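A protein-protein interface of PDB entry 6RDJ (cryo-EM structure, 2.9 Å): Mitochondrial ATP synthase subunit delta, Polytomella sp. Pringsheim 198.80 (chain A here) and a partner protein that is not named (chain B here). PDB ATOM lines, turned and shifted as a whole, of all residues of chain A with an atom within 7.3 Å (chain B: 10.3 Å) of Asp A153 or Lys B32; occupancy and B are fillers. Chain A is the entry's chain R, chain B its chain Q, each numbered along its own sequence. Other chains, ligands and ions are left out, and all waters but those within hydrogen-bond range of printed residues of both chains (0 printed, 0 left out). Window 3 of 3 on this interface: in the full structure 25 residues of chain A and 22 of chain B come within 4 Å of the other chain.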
ATOM      1  N   LYS A 126       3.127  -6.653   5.235  1.00  0.00           N
ATOM      2  CA  LYS A 126       4.577  -6.743   5.347  1.00  0.00           C
ATOM      3  C   LYS A 126       4.901  -7.322   6.716  1.00  0.00           C
ATOM      4  O   LYS A 126       4.972  -6.604   7.712  1.00  0.00           O
ATOM      5  CB  LYS A 126       5.230  -5.382   5.157  1.00  0.00           C
ATOM      6  CG  LYS A 126       4.891  -4.678   3.863  1.00  0.00           C
ATOM      7  CD  LYS A 126       5.189  -5.557   2.683  1.00  0.00           C
ATOM      8  CE  LYS A 126       5.288  -4.775   1.397  1.00  0.00           C
ATOM      9  NZ  LYS A 126       6.379  -3.767   1.474  1.00  0.00           N
ATOM     10  N   ALA A 150       6.851 -10.120  13.661  1.00  0.00           N
ATOM     11  CA  ALA A 150       6.260  -8.815  13.898  1.00  0.00           C
ATOM     12  C   ALA A 150       5.956  -8.116  12.582  1.00  0.00           C
ATOM     13  O   ALA A 150       6.731  -8.179  11.628  1.00  0.00           O
ATOM     14  CB  ALA A 150       7.202  -7.948  14.722  1.00  0.00           C
ATOM     15  N   THR A 151       4.820  -7.435  12.533  1.00  0.00           N
ATOM     16  CA  THR A 151       4.606  -6.561  11.394  1.00  0.00           C
ATOM     17  C   THR A 151       5.398  -5.274  11.597  1.00  0.00           C
ATOM     18  O   THR A 151       5.855  -4.960  12.696  1.00  0.00           O
ATOM     19  CB  THR A 151       3.119  -6.287  11.182  1.00  0.00           C
ATOM     20  OG1 THR A 151       2.907  -5.750   9.872  1.00  0.00           O
ATOM     21  CG2 THR A 151       2.611  -5.318  12.206  1.00  0.00           C
ATOM     22  N   LEU A 152       5.580  -4.527  10.511  1.00  0.00           N
ATOM     23  CA  LEU A 152       6.566  -3.455  10.513  1.00  0.00           C
ATOM     24  C   LEU A 152       6.109  -2.191  11.229  1.00  0.00           C
ATOM     25  O   LEU A 152       6.960  -1.371  11.587  1.00  0.00           O
ATOM     26  CB  LEU A 152       6.962  -3.125   9.077  1.00  0.00           C
ATOM     27  CG  LEU A 152       8.009  -4.095   8.545  1.00  0.00           C
ATOM     28  CD1 LEU A 152       8.085  -4.033   7.053  1.00  0.00           C
ATOM     29  CD2 LEU A 152       9.357  -3.765   9.150  1.00  0.00           C
ATOM     30  N   ASP A 153       4.808  -2.014  11.467  1.00  0.00           N
ATOM     31  CA  ASP A 153       4.353  -0.791  12.117  1.00  0.00           C
ATOM     32  C   ASP A 153       4.624  -0.807  13.616  1.00  0.00           C
ATOM     33  O   ASP A 153       4.791   0.255  14.224  1.00  0.00           O
ATOM     34  CB  ASP A 153       2.871  -0.548  11.819  1.00  0.00           C
ATOM     35  CG  ASP A 153       1.987  -1.749  12.122  1.00  0.00           C
ATOM     36  OD1 ASP A 153       1.159  -2.088  11.250  1.00  0.00           O
ATOM     37  OD2 ASP A 153       2.047  -2.308  13.237  1.00  0.00           O
ATOM     38  N   GLN A 154       4.663  -1.992  14.229  1.00  0.00           N
ATOM     39  CA  GLN A 154       4.876  -2.110  15.666  1.00  0.00           C
ATOM     40  C   GLN A 154       6.349  -2.258  16.019  1.00  0.00           C
ATOM     41  O   GLN A 154       6.686  -2.872  17.034  1.00  0.00           O
ATOM     42  CB  GLN A 154       4.068  -3.274  16.242  1.00  0.00           C
ATOM     43  CG  GLN A 154       4.323  -4.639  15.638  1.00  0.00           C
ATOM     44  CD  GLN A 154       3.122  -5.557  15.754  1.00  0.00           C
ATOM     45  OE1 GLN A 154       1.990  -5.146  15.524  1.00  0.00           O
ATOM     46  NE2 GLN A 154       3.363  -6.801  16.139  1.00  0.00           N
ATOM     47  N   VAL A 155       7.232  -1.695  15.203  1.00  0.00           N
ATOM     48  CA  VAL A 155       8.667  -1.702  15.457  1.00  0.00           C
ATOM     49  C   VAL A 155       9.094  -0.283  15.790  1.00  0.00           C
ATOM     50  O   VAL A 155       8.682   0.667  15.112  1.00  0.00           O
ATOM     51  CB  VAL A 155       9.449  -2.236  14.247  1.00  0.00           C
ATOM     52  CG1 VAL A 155      10.854  -2.620  14.662  1.00  0.00           C
ATOM     53  CG2 VAL A 155       8.722  -3.406  13.621  1.00  0.00           C
ATOM     54  N   ASP A 156       9.904  -0.136  16.837  1.00  0.00           N
ATOM     55  CA  ASP A 156      10.381   1.229  16.972  1.00  0.00           C
ATOM     56  C   ASP A 156      11.729   1.390  16.278  1.00  0.00           C
ATOM     57  O   ASP A 156      12.574   0.490  16.325  1.00  0.00           O
ATOM     58  CB  ASP A 156      10.501   1.618  18.446  1.00  0.00           C
ATOM     59  CG  ASP A 156      11.487   0.761  19.207  1.00  0.00           C
ATOM     60  OD1 ASP A 156      12.694   1.076  19.186  1.00  0.00           O
ATOM     61  OD2 ASP A 156      11.056  -0.221  19.840  1.00  0.00           O
ATOM     62  N   PRO A 157      11.961   2.513  15.605  1.00  0.00           N
ATOM     63  CA  PRO A 157      13.273   2.763  14.997  1.00  0.00           C
ATOM     64  C   PRO A 157      14.310   3.353  15.942  1.00  0.00           C
ATOM     65  O   PRO A 157      15.394   3.719  15.480  1.00  0.00           O
ATOM     66  CB  PRO A 157      12.930   3.764  13.890  1.00  0.00           C
ATOM     67  CG  PRO A 157      11.797   4.531  14.448  1.00  0.00           C
ATOM     68  CD  PRO A 157      10.989   3.565  15.265  1.00  0.00           C
ATOM     69  N   VAL A 195      13.054  -0.951   7.683  1.00  0.00           N
ATOM     70  CA  VAL A 195      12.254   0.098   8.299  1.00  0.00           C
ATOM     71  C   VAL A 195      12.632   1.492   7.794  1.00  0.00           C
ATOM     72  O   VAL A 195      11.790   2.403   7.860  1.00  0.00           O
ATOM     73  CB  VAL A 195      12.317   0.032   9.843  1.00  0.00           C
ATOM     74  CG1 VAL A 195      13.568   0.684  10.415  1.00  0.00           C
ATOM     75  CG2 VAL A 195      11.047   0.578  10.471  1.00  0.00           C
ATOM     76  N   LEU B  26      15.400 -11.096  20.330  1.00  0.00           N
ATOM     77  CA  LEU B  26      16.001  -9.853  19.878  1.00  0.00           C
ATOM     78  C   LEU B  26      15.053  -9.049  19.005  1.00  0.00           C
ATOM     79  O   LEU B  26      15.127  -7.818  19.002  1.00  0.00           O
ATOM     80  CB  LEU B  26      17.294 -10.167  19.138  1.00  0.00           C
ATOM     81  CG  LEU B  26      18.618 -10.006  19.860  1.00  0.00           C
ATOM     82  CD1 LEU B  26      18.554 -10.564  21.244  1.00  0.00           C
ATOM     83  CD2 LEU B  26      19.623 -10.785  19.084  1.00  0.00           C
ATOM     84  N   LEU B  27      14.170  -9.713  18.261  1.00  0.00           N
ATOM     85  CA  LEU B  27      13.084  -8.989  17.614  1.00  0.00           C
ATOM     86  C   LEU B  27      12.106  -8.438  18.641  1.00  0.00           C
ATOM     87  O   LEU B  27      11.551  -7.353  18.446  1.00  0.00           O
ATOM     88  CB  LEU B  27      12.353  -9.889  16.623  1.00  0.00           C
ATOM     89  CG  LEU B  27      11.231  -9.244  15.812  1.00  0.00           C
ATOM     90  CD1 LEU B  27      11.730  -7.981  15.159  1.00  0.00           C
ATOM     91  CD2 LEU B  27      10.682 -10.177  14.770  1.00  0.00           C
ATOM     92  N   ARG B  28      11.895  -9.157  19.742  1.00  0.00           N
ATOM     93  CA  ARG B  28      10.996  -8.656  20.774  1.00  0.00           C
ATOM     94  C   ARG B  28      11.596  -7.495  21.560  1.00  0.00           C
ATOM     95  O   ARG B  28      10.864  -6.592  21.973  1.00  0.00           O
ATOM     96  CB  ARG B  28      10.613  -9.784  21.730  1.00  0.00           C
ATOM     97  CG  ARG B  28       9.757 -10.855  21.106  1.00  0.00           C
ATOM     98  CD  ARG B  28       9.374 -11.896  22.127  1.00  0.00           C
ATOM     99  NE  ARG B  28       8.925 -13.122  21.488  1.00  0.00           N
ATOM    100  CZ  ARG B  28       9.597 -14.263  21.531  1.00  0.00           C
ATOM    101  NH1 ARG B  28      10.740 -14.332  22.189  1.00  0.00           N
ATOM    102  NH2 ARG B  28       9.123 -15.334  20.917  1.00  0.00           N
ATOM    103  N   ASN B  29      12.911  -7.483  21.763  1.00  0.00           N
ATOM    104  CA  ASN B  29      13.549  -6.455  22.575  1.00  0.00           C
ATOM    105  C   ASN B  29      13.652  -5.100  21.888  1.00  0.00           C
ATOM    106  O   ASN B  29      14.143  -4.154  22.509  1.00  0.00           O
ATOM    107  CB  ASN B  29      14.954  -6.902  22.991  1.00  0.00           C
ATOM    108  CG  ASN B  29      14.939  -7.880  24.142  1.00  0.00           C
ATOM    109  OD1 ASN B  29      15.671  -8.867  24.140  1.00  0.00           O
ATOM    110  ND2 ASN B  29      14.102  -7.613  25.137  1.00  0.00           N
ATOM    111  N   VAL B  30      13.247  -4.982  20.624  1.00  0.00           N
ATOM    112  CA  VAL B  30      13.201  -3.696  19.933  1.00  0.00           C
ATOM    113  C   VAL B  30      11.815  -3.505  19.341  1.00  0.00           C
ATOM    114  O   VAL B  30      11.625  -2.743  18.387  1.00  0.00           O
ATOM    115  CB  VAL B  30      14.290  -3.581  18.849  1.00  0.00           C
ATOM    116  CG1 VAL B  30      15.672  -3.613  19.474  1.00  0.00           C
ATOM    117  CG2 VAL B  30      14.157  -4.709  17.840  1.00  0.00           C
ATOM    118  N   LEU B  31      10.838  -4.187  19.911  1.00  0.00           N
ATOM    119  CA  LEU B  31       9.457  -4.016  19.501  1.00  0.00           C
ATOM    120  C   LEU B  31       8.886  -2.773  20.182  1.00  0.00           C
ATOM    121  O   LEU B  31       9.419  -2.292  21.185  1.00  0.00           O
ATOM    122  CB  LEU B  31       8.658  -5.267  19.866  1.00  0.00           C
ATOM    123  CG  LEU B  31       7.325  -5.583  19.197  1.00  0.00           C
ATOM    124  CD1 LEU B  31       7.567  -5.925  17.770  1.00  0.00           C
ATOM    125  CD2 LEU B  31       6.666  -6.746  19.894  1.00  0.00           C
ATOM    126  N   LYS B  32       7.802  -2.243  19.610  1.00  0.00           N
ATOM    127  CA  LYS B  32       7.134  -1.078  20.180  1.00  0.00           C
ATOM    128  C   LYS B  32       6.513  -1.421  21.531  1.00  0.00           C
ATOM    129  O   LYS B  32       5.875  -2.466  21.685  1.00  0.00           O
ATOM    130  CB  LYS B  32       6.053  -0.567  19.233  1.00  0.00           C
ATOM    131  CG  LYS B  32       5.520   0.808  19.563  1.00  0.00           C
ATOM    132  CD  LYS B  32       6.556   1.881  19.310  1.00  0.00           C
ATOM    133  CE  LYS B  32       6.785   2.077  17.823  1.00  0.00           C
ATOM    134  NZ  LYS B  32       5.547   2.484  17.109  1.00  0.00           N
ATOM    135  N   GLU B  33       6.693  -0.516  22.496  1.00  0.00           N
ATOM    136  CA  GLU B  33       6.340  -0.788  23.890  1.00  0.00           C
ATOM    137  C   GLU B  33       4.858  -1.084  24.164  1.00  0.00           C
ATOM    138  O   GLU B  33       4.596  -1.874  25.090  1.00  0.00           O
ATOM    139  CB  GLU B  33       6.866   0.378  24.754  1.00  0.00           C
ATOM    140  CG  GLU B  33       6.536   0.333  26.240  1.00  0.00           C
ATOM    141  CD  GLU B  33       7.312  -0.751  26.977  1.00  0.00           C
ATOM    142  OE1 GLU B  33       8.551  -0.811  26.827  1.00  0.00           O
ATOM    143  OE2 GLU B  33       6.676  -1.546  27.702  1.00  0.00           O
ATOM    144  N   PRO B  34       3.866  -0.545  23.427  1.00  0.00           N
ATOM    145  CA  PRO B  34       2.506  -1.110  23.539  1.00  0.00           C
ATOM    146  C   PRO B  34       2.391  -2.593  23.216  1.00  0.00           C
ATOM    147  O   PRO B  34       1.481  -3.250  23.735  1.00  0.00           O
ATOM    148  CB  PRO B  34       1.705  -0.265  22.544  1.00  0.00           C
ATOM    149  CG  PRO B  34       2.332   1.052  22.647  1.00  0.00           C
ATOM    150  CD  PRO B  34       3.798   0.814  22.849  1.00  0.00           C
ATOM    151  N   PHE B  35       3.279  -3.145  22.384  1.00  0.00           N
ATOM    152  CA  PHE B  35       3.315  -4.576  22.124  1.00  0.00           C
ATOM    153  C   PHE B  35       4.529  -5.280  22.709  1.00  0.00           C
ATOM    154  O   PHE B  35       4.485  -6.503  22.879  1.00  0.00           O
ATOM    155  CB  PHE B  35       3.280  -4.843  20.617  1.00  0.00           C
ATOM    156  CG  PHE B  35       2.049  -4.333  19.939  1.00  0.00           C
ATOM    157  CD1 PHE B  35       0.861  -5.038  20.015  1.00  0.00           C
ATOM    158  CD2 PHE B  35       2.080  -3.155  19.216  1.00  0.00           C
ATOM    159  CE1 PHE B  35      -0.275  -4.577  19.383  1.00  0.00           C
ATOM    160  CE2 PHE B  35       0.951  -2.688  18.578  1.00  0.00           C
ATOM    161  CZ  PHE B  35      -0.230  -3.401  18.662  1.00  0.00           C
ATOM    162  N   LYS B  36       5.601  -4.540  23.012  1.00  0.00           N
ATOM    163  CA  LYS B  36       6.834  -5.146  23.510  1.00  0.00           C
ATOM    164  C   LYS B  36       6.631  -5.794  24.869  1.00  0.00           C
ATOM    165  O   LYS B  36       7.171  -6.874  25.128  1.00  0.00           O
ATOM    166  CB  LYS B  36       7.939  -4.094  23.587  1.00  0.00           C
ATOM    167  CG  LYS B  36       9.249  -4.560  24.195  1.00  0.00           C
ATOM    168  CD  LYS B  36      10.257  -3.426  24.237  1.00  0.00           C
ATOM    169  CE  LYS B  36      11.571  -3.872  24.840  1.00  0.00           C
ATOM    170  NZ  LYS B  36      11.386  -4.394  26.214  1.00  0.00           N
ATOM    171  N   ALA B  37       5.827  -5.172  25.733  1.00  0.00           N
ATOM    172  CA  ALA B  37       5.635  -5.703  27.079  1.00  0.00           C
ATOM    173  C   ALA B  37       4.813  -6.982  27.060  1.00  0.00           C
ATOM    174  O   ALA B  37       5.136  -7.943  27.766  1.00  0.00           O
ATOM    175  CB  ALA B  37       4.965  -4.655  27.966  1.00  0.00           C
ATOM    176  N   LYS B  38       3.758  -7.026  26.253  1.00  0.00           N
ATOM    177  CA  LYS B  38       2.975  -8.245  26.149  1.00  0.00           C
ATOM    178  C   LYS B  38       3.659  -9.306  25.297  1.00  0.00           C
ATOM    179  O   LYS B  38       3.246 -10.469  25.335  1.00  0.00           O
ATOM    180  CB  LYS B  38       1.587  -7.935  25.597  1.00  0.00           C
ATOM    181  CG  LYS B  38       1.593  -7.188  24.287  1.00  0.00           C
ATOM    182  CD  LYS B  38       0.187  -7.034  23.748  1.00  0.00           C
ATOM    183  CE  LYS B  38      -0.470  -8.389  23.552  1.00  0.00           C
ATOM    184  NZ  LYS B  38       0.370  -9.310  22.737  1.00  0.00           N
ATOM    185  N   ALA B  39       4.687  -8.941  24.538  1.00  0.00           N
ATOM    186  CA  ALA B  39       5.565  -9.939  23.953  1.00  0.00           C
ATOM    187  C   ALA B  39       6.591 -10.472  24.945  1.00  0.00           C
ATOM    188  O   ALA B  39       7.227 -11.488  24.663  1.00  0.00           O
ATOM    189  CB  ALA B  39       6.284  -9.362  22.735  1.00  0.00           C
ATOM    190  N   GLN B  40       6.767  -9.822  26.099  1.00  0.00           N
ATOM    191  CA  GLN B  40       7.567 -10.416  27.166  1.00  0.00           C
ATOM    192  C   GLN B  40       6.797 -11.458  27.958  1.00  0.00           C
ATOM    193  O   GLN B  40       7.369 -12.061  28.871  1.00  0.00           O
ATOM    194  CB  GLN B  40       8.095  -9.353  28.127  1.00  0.00           C
ATOM    195  CG  GLN B  40       8.865  -8.233  27.470  1.00  0.00           C
ATOM    196  CD  GLN B  40      10.359  -8.429  27.528  1.00  0.00           C
ATOM    197  OE1 GLN B  40      10.847  -9.554  27.615  1.00  0.00           O
ATOM    198  NE2 GLN B  40      11.100  -7.332  27.471  1.00  0.00           N
ATOM    199  N   ARG B  42       5.420 -14.189  26.355  1.00  0.00           N
ATOM    200  CA  ARG B  42       5.940 -15.381  25.705  1.00  0.00           C
ATOM    201  C   ARG B  42       7.459 -15.413  25.642  1.00  0.00           C
ATOM    202  O   ARG B  42       8.017 -16.330  25.038  1.00  0.00           O
ATOM    203  CB  ARG B  42       5.357 -15.510  24.304  1.00  0.00           C
ATOM    204  CG  ARG B  42       5.777 -14.437  23.372  1.00  0.00           C
ATOM    205  CD  ARG B  42       4.663 -14.155  22.422  1.00  0.00           C
ATOM    206  NE  ARG B  42       5.052 -13.184  21.415  1.00  0.00           N
ATOM    207  CZ  ARG B  42       4.185 -12.471  20.712  1.00  0.00           C
ATOM    208  NH1 ARG B  42       4.618 -11.612  19.804  1.00  0.00           N
ATOM    209  NH2 ARG B  42       2.886 -12.623  20.913  1.00  0.00           N
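Hydrophobic or aromatic side chains of chain B that line the printed part of chain A: Leu B27, Leu B31 and Phe B35. Along chain B the printed residues that touch a printed residue of chain A span positions 27 to 35. Of the 10 printed residues of chain A, 5 touch a printed residue of chain B.
The side-chain carboxylate (OD2) of Asp A156 sits close to the backbone carbonyl oxygen (O) of Leu B31, 3.0 Å away. N of Lys B32 sits at hydrogen-bond distance from O of Gln A154, at 2.9 Å. The backbone NH (N) of Asp A156 is in hydrogen-bond range of the backbone carbonyl oxygen (O) of Val B30 (3.5 Å).
Asp A153 touches just one residue of chain B: Lys B32 (3.7 Å). Of chain A, only Asp A153, Gln A154, Val A155 and Asp A156 come within 4 Å of Lys B32. No residue of chain B comes within 4 Å of Leu A152. Of chain B, only Leu B31, Lys B32 and Phe B35 come within 4 Å of Gln A154. Val A155 touches two residues of chain B. Printed residues of chain A within 4 Å of Leu B31: Ala A150, Gln A154 and Asp A156. Printed residues of chain A within 4 Å of Val B30: Val A155 (3.8 Å) and Asp A156 (3.0 Å). Of the printed residues of chain A, Phe B35 touches Gln A154. Of the printed residues of chain A, Leu B27 touches Ala A150. Leu B26 touches none of the printed residues of chain A. Pro A157 touches none of the printed residues of chain B. The nearest residue of chain B that does not touch Asp A153 is Phe B35 (5.5 Å). The nearest residue of chain A that does not touch Lys B32 is Pro A157 (5.1 Å).
Ala A150 touches Leu B27. Ala A150 touches Leu B31. Asp A153 touches Lys B32 (O to NZ, 3.7 Å). Leu B31 touches Gln A154. CD2 of Phe B35 touches CB of Gln A154, at 3.6 Å. CG1 of Val A155 touches O of Val B30 (3.8 Å). Val A155 touches Lys B32 (O to CE, 3.6 Å). Asp A156 touches Lys B32.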
